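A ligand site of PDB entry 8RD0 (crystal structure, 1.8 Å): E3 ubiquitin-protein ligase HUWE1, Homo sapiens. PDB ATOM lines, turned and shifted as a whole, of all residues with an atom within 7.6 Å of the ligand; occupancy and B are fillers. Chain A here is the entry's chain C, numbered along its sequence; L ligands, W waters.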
ATOM      1  N   TRP A  10      32.606  11.558  19.007  1.00  0.00           N
ATOM      2  CA  TRP A  10      32.716  10.148  18.638  1.00  0.00           C
ATOM      3  C   TRP A  10      34.156   9.897  18.216  1.00  0.00           C
ATOM      4  O   TRP A  10      34.772  10.777  17.624  1.00  0.00           O
ATOM      5  CB  TRP A  10      31.727   9.765  17.539  1.00  0.00           C
ATOM      6  CG  TRP A  10      31.879  10.494  16.242  1.00  0.00           C
ATOM      7  CD1 TRP A  10      31.311  11.687  15.903  1.00  0.00           C
ATOM      8  CD2 TRP A  10      32.585  10.038  15.093  1.00  0.00           C
ATOM      9  NE1 TRP A  10      31.641  12.011  14.609  1.00  0.00           N
ATOM     10  CE2 TRP A  10      32.399  11.007  14.078  1.00  0.00           C
ATOM     11  CE3 TRP A  10      33.370   8.925  14.812  1.00  0.00           C
ATOM     12  CZ2 TRP A  10      33.012  10.899  12.833  1.00  0.00           C
ATOM     13  CZ3 TRP A  10      33.931   8.800  13.563  1.00  0.00           C
ATOM     14  CH2 TRP A  10      33.757   9.771  12.591  1.00  0.00           C
ATOM     15  N   PHE A  11      34.712   8.714  18.539  1.00  0.00           N
ATOM     16  CA  PHE A  11      36.107   8.431  18.186  1.00  0.00           C
ATOM     17  C   PHE A  11      36.227   7.801  16.815  1.00  0.00           C
ATOM     18  O   PHE A  11      35.539   6.842  16.516  1.00  0.00           O
ATOM     19  CB  PHE A  11      36.787   7.533  19.216  1.00  0.00           C
ATOM     20  CG  PHE A  11      38.294   7.457  19.076  1.00  0.00           C
ATOM     21  CD1 PHE A  11      39.089   8.493  19.528  1.00  0.00           C
ATOM     22  CD2 PHE A  11      38.899   6.352  18.514  1.00  0.00           C
ATOM     23  CE1 PHE A  11      40.464   8.412  19.434  1.00  0.00           C
ATOM     24  CE2 PHE A  11      40.282   6.281  18.427  1.00  0.00           C
ATOM     25  CZ  PHE A  11      41.054   7.318  18.889  1.00  0.00           C
ATOM     26  N   ASP A  12      37.138   8.343  15.986  1.00  0.00           N
ATOM     27  CA  ASP A  12      37.423   7.811  14.681  1.00  0.00           C
ATOM     28  C   ASP A  12      38.706   6.983  14.746  1.00  0.00           C
ATOM     29  O   ASP A  12      39.786   7.554  14.853  1.00  0.00           O
ATOM     30  CB  ASP A  12      37.566   8.967  13.692  1.00  0.00           C
ATOM     31  CG  ASP A  12      37.616   8.531  12.241  1.00  0.00           C
ATOM     32  OD1 ASP A  12      37.873   7.326  11.988  1.00  0.00           O
ATOM     33  OD2 ASP A  12      37.377   9.385  11.368  1.00  0.00           O
ATOM     34  N   ARG A  14      40.186   5.395  12.387  1.00  0.00           N
ATOM     35  CA  ARG A  14      40.953   5.487  11.149  1.00  0.00           C
ATOM     36  C   ARG A  14      41.997   6.603  11.334  1.00  0.00           C
ATOM     37  O   ARG A  14      43.160   6.406  10.983  1.00  0.00           O
ATOM     38  CB  ARG A  14      40.045   5.799   9.948  1.00  0.00           C
ATOM     39  CG  ARG A  14      38.939   4.775   9.687  1.00  0.00           C
ATOM     40  CD  ARG A  14      37.835   5.326   8.782  1.00  0.00           C
ATOM     41  NE  ARG A  14      37.066   6.404   9.399  1.00  0.00           N
ATOM     42  CZ  ARG A  14      36.103   7.101   8.791  1.00  0.00           C
ATOM     43  NH1 ARG A  14      35.775   6.827   7.526  1.00  0.00           N
ATOM     44  NH2 ARG A  14      35.468   8.065   9.429  1.00  0.00           N
ATOM     45  N   CYS A  19      36.041  13.235  17.331  1.00  0.00           N
ATOM     46  CA  CYS A  19      35.403  14.087  16.334  1.00  0.00           C
ATOM     47  C   CYS A  19      34.153  14.736  16.915  1.00  0.00           C
ATOM     48  O   CYS A  19      33.380  14.074  17.602  1.00  0.00           O
ATOM     49  CB  CYS A  19      35.024  13.266  15.113  1.00  0.00           C
ATOM     50  SG  CYS A  19      36.402  12.319  14.407  1.00  0.00           S
ATOM     51  N   SER A  20      33.901  15.990  16.561  1.00  0.00           N
ATOM     52  CA  SER A  20      32.701  16.703  16.958  1.00  0.00           C
ATOM     53  C   SER A  20      31.541  16.346  16.011  1.00  0.00           C
ATOM     54  O   SER A  20      31.744  16.030  14.837  1.00  0.00           O
ATOM     55  CB  SER A  20      32.922  18.221  16.861  1.00  0.00           C
ATOM     56  OG  SER A  20      33.860  18.640  17.832  1.00  0.00           O
ATOM     57  N   TYR A  21      30.329  16.471  16.528  1.00  0.00           N
ATOM     58  CA  TYR A  21      29.129  16.324  15.714  1.00  0.00           C
ATOM     59  C   TYR A  21      28.756  17.705  15.168  1.00  0.00           C
ATOM     60  O   TYR A  21      29.186  18.735  15.719  1.00  0.00           O
ATOM     61  CB  TYR A  21      27.969  15.815  16.580  1.00  0.00           C
ATOM     62  CG  TYR A  21      28.113  14.366  17.002  1.00  0.00           C
ATOM     63  CD1 TYR A  21      27.668  13.343  16.172  1.00  0.00           C
ATOM     64  CD2 TYR A  21      28.621  14.016  18.239  1.00  0.00           C
ATOM     65  CE1 TYR A  21      27.794  12.010  16.550  1.00  0.00           C
ATOM     66  CE2 TYR A  21      28.741  12.694  18.622  1.00  0.00           C
ATOM     67  CZ  TYR A  21      28.305  11.690  17.784  1.00  0.00           C
ATOM     68  OH  TYR A  21      28.369  10.380  18.173  1.00  0.00           O
ATOM     69  N   SER A  22      27.882  17.760  14.154  1.00  0.00           N
ATOM     70  CA  SER A  22      27.349  19.036  13.667  1.00  0.00           C
ATOM     71  C   SER A  22      26.501  19.654  14.795  1.00  0.00           C
ATOM     72  O   SER A  22      26.070  18.928  15.680  1.00  0.00           O
ATOM     73  CB  SER A  22      26.469  18.823  12.446  1.00  0.00           C
ATOM     74  OG  SER A  22      25.272  18.120  12.762  1.00  0.00           O
ATOM     75  N   ASN A  25      23.108  17.684  14.986  1.00  0.00           N
ATOM     76  CA  ASN A  25      23.188  16.308  15.528  1.00  0.00           C
ATOM     77  C   ASN A  25      23.599  16.325  16.979  1.00  0.00           C
ATOM     78  O   ASN A  25      23.047  15.561  17.792  1.00  0.00           O
ATOM     79  CB  ASN A  25      24.115  15.445  14.680  1.00  0.00           C
ATOM     80  CG  ASN A  25      23.510  15.127  13.311  1.00  0.00           C
ATOM     81  OD1 ASN A  25      22.295  15.150  13.147  1.00  0.00           O
ATOM     82  ND2 ASN A  25      24.316  14.818  12.326  1.00  0.00           N
ATOM     83  N   ILE A  29      21.349  14.702  20.030  1.00  0.00           N
ATOM     84  CA  ILE A  29      21.952  13.794  21.030  1.00  0.00           C
ATOM     85  C   ILE A  29      21.794  14.374  22.447  1.00  0.00           C
ATOM     86  O   ILE A  29      21.288  13.689  23.345  1.00  0.00           O
ATOM     87  CB  ILE A  29      23.429  13.492  20.698  1.00  0.00           C
ATOM     88  CG1 ILE A  29      23.563  12.703  19.346  1.00  0.00           C
ATOM     89  CG2 ILE A  29      24.094  12.709  21.851  1.00  0.00           C
ATOM     90  CD1 ILE A  29      24.910  12.827  18.682  1.00  0.00           C
ATOM     91  N   PHE A  42      20.050   9.609  15.085  1.00  0.00           N
ATOM     92  CA  PHE A  42      20.261  10.784  14.277  1.00  0.00           C
ATOM     93  C   PHE A  42      20.757  10.344  12.886  1.00  0.00           C
ATOM     94  O   PHE A  42      21.224   9.220  12.729  1.00  0.00           O
ATOM     95  CB  PHE A  42      21.250  11.771  14.929  1.00  0.00           C
ATOM     96  CG  PHE A  42      22.685  11.316  14.932  1.00  0.00           C
ATOM     97  CD1 PHE A  42      23.531  11.613  13.875  1.00  0.00           C
ATOM     98  CD2 PHE A  42      23.179  10.523  15.956  1.00  0.00           C
ATOM     99  CE1 PHE A  42      24.804  11.093  13.819  1.00  0.00           C
ATOM    100  CE2 PHE A  42      24.470  10.044  15.925  1.00  0.00           C
ATOM    101  CZ  PHE A  42      25.288  10.340  14.857  1.00  0.00           C
ATOM    102  N   THR A  43      20.646  11.251  11.901  1.00  0.00           N
ATOM    103  CA  THR A  43      21.061  10.976  10.533  1.00  0.00           C
ATOM    104  C   THR A  43      22.233  11.868  10.106  1.00  0.00           C
ATOM    105  O   THR A  43      22.214  13.060  10.412  1.00  0.00           O
ATOM    106  CB  THR A  43      19.846  11.211   9.619  1.00  0.00           C
ATOM    107  OG1 THR A  43      18.775  10.311  10.028  1.00  0.00           O
ATOM    108  CG2 THR A  43      20.173  11.049   8.175  1.00  0.00           C
ATOM    109  N   ALA A  44      23.178  11.307   9.338  1.00  0.00           N
ATOM    110  CA  ALA A  44      24.287  12.067   8.741  1.00  0.00           C
ATOM    111  C   ALA A  44      24.796  11.362   7.496  1.00  0.00           C
ATOM    112  O   ALA A  44      25.062  10.177   7.564  1.00  0.00           O
ATOM    113  CB  ALA A  44      25.427  12.234   9.732  1.00  0.00           C
ATOM    114  N   GLY A  45      24.919  12.063   6.366  1.00  0.00           N
ATOM    115  CA  GLY A  45      25.510  11.504   5.143  1.00  0.00           C
ATOM    116  C   GLY A  45      24.984  10.157   4.672  1.00  0.00           C
ATOM    117  O   GLY A  45      25.778   9.256   4.326  1.00  0.00           O
ATOM    118  N   ARG A  47      23.324   7.941   6.339  1.00  0.00           N
ATOM    119  CA  ARG A  47      23.436   6.889   7.336  1.00  0.00           C
ATOM    120  C   ARG A  47      22.684   7.313   8.588  1.00  0.00           C
ATOM    121  O   ARG A  47      22.691   8.469   8.977  1.00  0.00           O
ATOM    122  CB  ARG A  47      24.933   6.576   7.649  1.00  0.00           C
ATOM    123  CG  ARG A  47      25.797   6.245   6.398  1.00  0.00           C
ATOM    124  CD  ARG A  47      25.713   4.840   5.937  1.00  0.00           C
ATOM    125  NE  ARG A  47      25.855   4.663   4.466  1.00  0.00           N
ATOM    126  CZ  ARG A  47      26.992   4.536   3.784  1.00  0.00           C
ATOM    127  NH1 ARG A  47      26.965   4.300   2.482  1.00  0.00           N
ATOM    128  NH2 ARG A  47      28.168   4.611   4.399  1.00  0.00           N
ATOM    129  N   TYR A  49      22.355   6.561  12.662  1.00  0.00           N
ATOM    130  CA  TYR A  49      23.155   6.093  13.780  1.00  0.00           C
ATOM    131  C   TYR A  49      22.319   6.098  15.049  1.00  0.00           C
ATOM    132  O   TYR A  49      21.460   6.953  15.207  1.00  0.00           O
ATOM    133  CB  TYR A  49      24.345   7.040  14.022  1.00  0.00           C
ATOM    134  CG  TYR A  49      25.284   7.170  12.857  1.00  0.00           C
ATOM    135  CD1 TYR A  49      26.458   6.426  12.793  1.00  0.00           C
ATOM    136  CD2 TYR A  49      25.056   8.095  11.851  1.00  0.00           C
ATOM    137  CE1 TYR A  49      27.348   6.565  11.733  1.00  0.00           C
ATOM    138  CE2 TYR A  49      25.902   8.209  10.758  1.00  0.00           C
ATOM    139  CZ  TYR A  49      27.042   7.423  10.692  1.00  0.00           C
ATOM    140  OH  TYR A  49      27.878   7.569   9.595  1.00  0.00           O
ATOM    141  N   GLN A  58      28.139   4.482  19.743  1.00  0.00           N
ATOM    142  CA  GLN A  58      27.367   4.867  18.576  1.00  0.00           C
ATOM    143  C   GLN A  58      27.369   3.650  17.631  1.00  0.00           C
ATOM    144  O   GLN A  58      28.432   3.088  17.328  1.00  0.00           O
ATOM    145  CB  GLN A  58      28.004   6.081  17.896  1.00  0.00           C
ATOM    146  CG  GLN A  58      27.339   6.503  16.592  1.00  0.00           C
ATOM    147  CD  GLN A  58      28.222   7.493  15.852  1.00  0.00           C
ATOM    148  OE1 GLN A  58      28.065   8.697  16.019  1.00  0.00           O
ATOM    149  NE2 GLN A  58      29.164   7.001  15.063  1.00  0.00           N
ATOM    150  N   VAL A  59      26.195   3.262  17.140  1.00  0.00           N
ATOM    151  CA  VAL A  59      26.057   2.137  16.228  1.00  0.00           C
ATOM    152  C   VAL A  59      25.582   2.682  14.879  1.00  0.00           C
ATOM    153  O   VAL A  59      24.543   3.351  14.812  1.00  0.00           O
ATOM    154  CB  VAL A  59      25.051   1.088  16.762  1.00  0.00           C
ATOM    155  CG1 VAL A  59      24.971  -0.102  15.815  1.00  0.00           C
ATOM    156  CG2 VAL A  59      25.413   0.653  18.191  1.00  0.00           C
ATOM    157  N   ASN A  60      26.313   2.359  13.822  1.00  0.00           N
ATOM    158  CA  ASN A  60      25.942   2.710  12.465  1.00  0.00           C
ATOM    159  C   ASN A  60      24.873   1.691  12.091  1.00  0.00           C
ATOM    160  O   ASN A  60      25.168   0.494  12.022  1.00  0.00           O
ATOM    161  CB  ASN A  60      27.169   2.605  11.554  1.00  0.00           C
ATOM    162  CG  ASN A  60      26.901   2.993  10.125  1.00  0.00           C
ATOM    163  OD1 ASN A  60      25.887   2.619   9.529  1.00  0.00           O
ATOM    164  ND2 ASN A  60      27.828   3.726   9.527  1.00  0.00           N
ATOM    165  N   THR A  63      25.698  -0.320   8.578  1.00  0.00           N
ATOM    166  CA  THR A  63      26.782  -1.298   8.556  1.00  0.00           C
ATOM    167  C   THR A  63      26.909  -2.163   9.809  1.00  0.00           C
ATOM    168  O   THR A  63      27.492  -3.237   9.729  1.00  0.00           O
ATOM    169  CB  THR A  63      28.119  -0.571   8.340  1.00  0.00           C
ATOM    170  OG1 THR A  63      28.430   0.197   9.508  1.00  0.00           O
ATOM    171  CG2 THR A  63      28.114   0.315   7.123  1.00  0.00           C
ATOM    172  N   ASN A  65      28.657  -1.042  12.368  1.00  0.00           N
ATOM    173  CA  ASN A  65      29.889  -0.622  13.000  1.00  0.00           C
ATOM    174  C   ASN A  65      29.654   0.175  14.282  1.00  0.00           C
ATOM    175  O   ASN A  65      28.820   1.099  14.308  1.00  0.00           O
ATOM    176  CB  ASN A  65      30.757   0.181  12.039  1.00  0.00           C
ATOM    177  CG  ASN A  65      32.149   0.386  12.551  1.00  0.00           C
ATOM    178  OD1 ASN A  65      32.848  -0.579  12.851  1.00  0.00           O
ATOM    179  ND2 ASN A  65      32.599   1.617  12.644  1.00  0.00           N
ATOM    180  N   ARG A  66      30.439  -0.126  15.311  1.00  0.00           N
ATOM    181  CA  ARG A  66      30.329   0.501  16.628  1.00  0.00           C
ATOM    182  C   ARG A  66      31.515   1.419  16.873  1.00  0.00           C
ATOM    183  O   ARG A  66      32.662   0.992  16.651  1.00  0.00           O
ATOM    184  CB  ARG A  66      30.287  -0.605  17.693  1.00  0.00           C
ATOM    185  CG  ARG A  66      29.058  -1.490  17.620  1.00  0.00           C
ATOM    186  CD  ARG A  66      29.174  -2.762  18.466  1.00  0.00           C
ATOM    187  NE  ARG A  66      29.349  -2.487  19.884  1.00  0.00           N
ATOM    188  CZ  ARG A  66      28.375  -2.158  20.737  1.00  0.00           C
ATOM    189  NH1 ARG A  66      28.669  -1.918  22.017  1.00  0.00           N
ATOM    190  NH2 ARG A  66      27.118  -2.042  20.319  1.00  0.00           N
ATOM    191  N   ARG A  67      31.248   2.661  17.253  1.00  0.00           N
ATOM    192  CA  ARG A  67      32.279   3.644  17.588  1.00  0.00           C
ATOM    193  C   ARG A  67      31.978   4.195  18.961  1.00  0.00           C
ATOM    194  O   ARG A  67      30.817   4.496  19.264  1.00  0.00           O
ATOM    195  CB  ARG A  67      32.315   4.787  16.583  1.00  0.00           C
ATOM    196  CG  ARG A  67      32.782   4.302  15.202  1.00  0.00           C
ATOM    197  CD  ARG A  67      33.019   5.429  14.250  1.00  0.00           C
ATOM    198  NE  ARG A  67      33.125   5.007  12.849  1.00  0.00           N
ATOM    199  CZ  ARG A  67      34.242   4.683  12.193  1.00  0.00           C
ATOM    200  NH1 ARG A  67      35.420   4.667  12.817  1.00  0.00           N
ATOM    201  NH2 ARG A  67      34.189   4.363  10.907  1.00  0.00           N
HETATM  202  C1  LIG L   1      31.350   6.243   9.215  1.00  0.00           C
HETATM  203  C2  LIG L   1      31.966   7.229  10.196  1.00  0.00           C
HETATM  204  C3  LIG L   1      30.523   8.366  11.916  1.00  0.00           C
HETATM  205  C4  LIG L   1      29.762   9.642  11.944  1.00  0.00           C
HETATM  206  C5  LIG L   1      29.009  10.217  12.961  1.00  0.00           C
HETATM  207  C6  LIG L   1      28.396  11.445  12.716  1.00  0.00           C
HETATM  208  C7  LIG L   1      28.514  12.049  11.477  1.00  0.00           C
HETATM  209  C8  LIG L   1      29.243  11.453  10.459  1.00  0.00           C
HETATM  210  C9  LIG L   1      29.880  10.250  10.714  1.00  0.00           C
HETATM  211  C10 LIG L   1      30.706   9.378   9.847  1.00  0.00           C
HETATM  212  O1  LIG L   1      32.157   5.417   8.713  1.00  0.00           O
HETATM  213  N1  LIG L   1      31.057   8.285  10.634  1.00  0.00           N
HETATM  214  O2  LIG L   1      31.017   9.510   8.675  1.00  0.00           O
HETATM  215  O3  LIG L   1      30.720   7.584  12.810  1.00  0.00           O
HETATM  216  O4  LIG L   1      30.127   6.275   8.969  1.00  0.00           O
HETATM  217  O   HOH W   1      28.990   4.280   6.821  1.00  0.00           O
HETATM  218  O   HOH W   2      27.487  15.063  12.702  1.00  0.00           O
HETATM  219  O   HOH W   3      30.706  14.269  13.044  1.00  0.00           O
HETATM  220  O   HOH W   4      32.733   4.299   6.447  1.00  0.00           O
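OH of Tyr 49 sits at hydrogen-bond distance from O4 of the ligand, at 2.7 Å.
O3 of the ligand is in hydrogen-bond range of NE2 of Gln 58, 2.8 Å away.
The side-chain amide nitrogen of Asn 60 is in hydrogen-bond range of an oxygen (O4) of the ligand (3.5 Å).
The guanidinium group of Arg 67 is in salt-bridge range of an oxygen (O1) of the ligand, at 3.2 Å.
Water W1 lies within hydrogen-bond range of NH2 of Arg 47 (2.6 Å), ND2 of Asn 60 (3.0 Å) and O4 of the ligand (3.1 Å).
Water W2 bridges the backbone NH of Ser 22 (3.1 Å) and the side-chain amide nitrogen of Asn 25 (3.2 Å).
Water W3 lies within hydrogen-bond range of O of Ser 20 (2.7 Å) and NE1 of Trp 10 (2.9 Å).
O of Arg 67 lies within hydrogen-bond range of N of Gln 58 (2.7 Å).
NH1 of Arg 67 is in salt-bridge range of OD1 of Asp 12.
The side-chain amide oxygen (OE1) of Gln 58 lies within hydrogen-bond range of the side-chain hydroxyl (OH) of Tyr 21.
The guanidinium group (NE) of Arg 14 is in salt-bridge range of the side-chain carboxylate (OD1) of Asp 12, 2.9 Å away.
OD1 of Asn 60 sits at hydrogen-bond distance from N of Thr 63 (3.1 Å).
The guanidinium group of Arg 67 lies close to the side-chain amide nitrogen of Asn 65 (3.4 Å).
The backbone carbonyl oxygen (O) of Trp 10 sits at hydrogen-bond distance from the backbone NH (N) of Cys 19, 2.8 Å away.
The backbone carbonyl oxygen (O) of Phe 42 sits at hydrogen-bond distance from the backbone NH (N) of Tyr 49, at 2.9 Å.
Trp 10 touches the ligand (CZ3 to O3, 3.5 Å).
Arg 14 touches the ligand (NH2 to C2, 3.7 Å).
Tyr 21 touches the ligand.
CE1 of Phe 42 touches C6 of the ligand (3.8 Å).
Ala 44 touches the ligand (CB to C7, 3.6 Å).
Hydrophobic or aromatic side chains that line the ligand: Trp 10, Tyr 21, Phe 42, Ala 44 and Tyr 49.
Of the 23 residues printed, 9 come within 4 Å of the ligand.
The nearest printed residue that does not touch the ligand is Arg 47 (5.0 Å).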
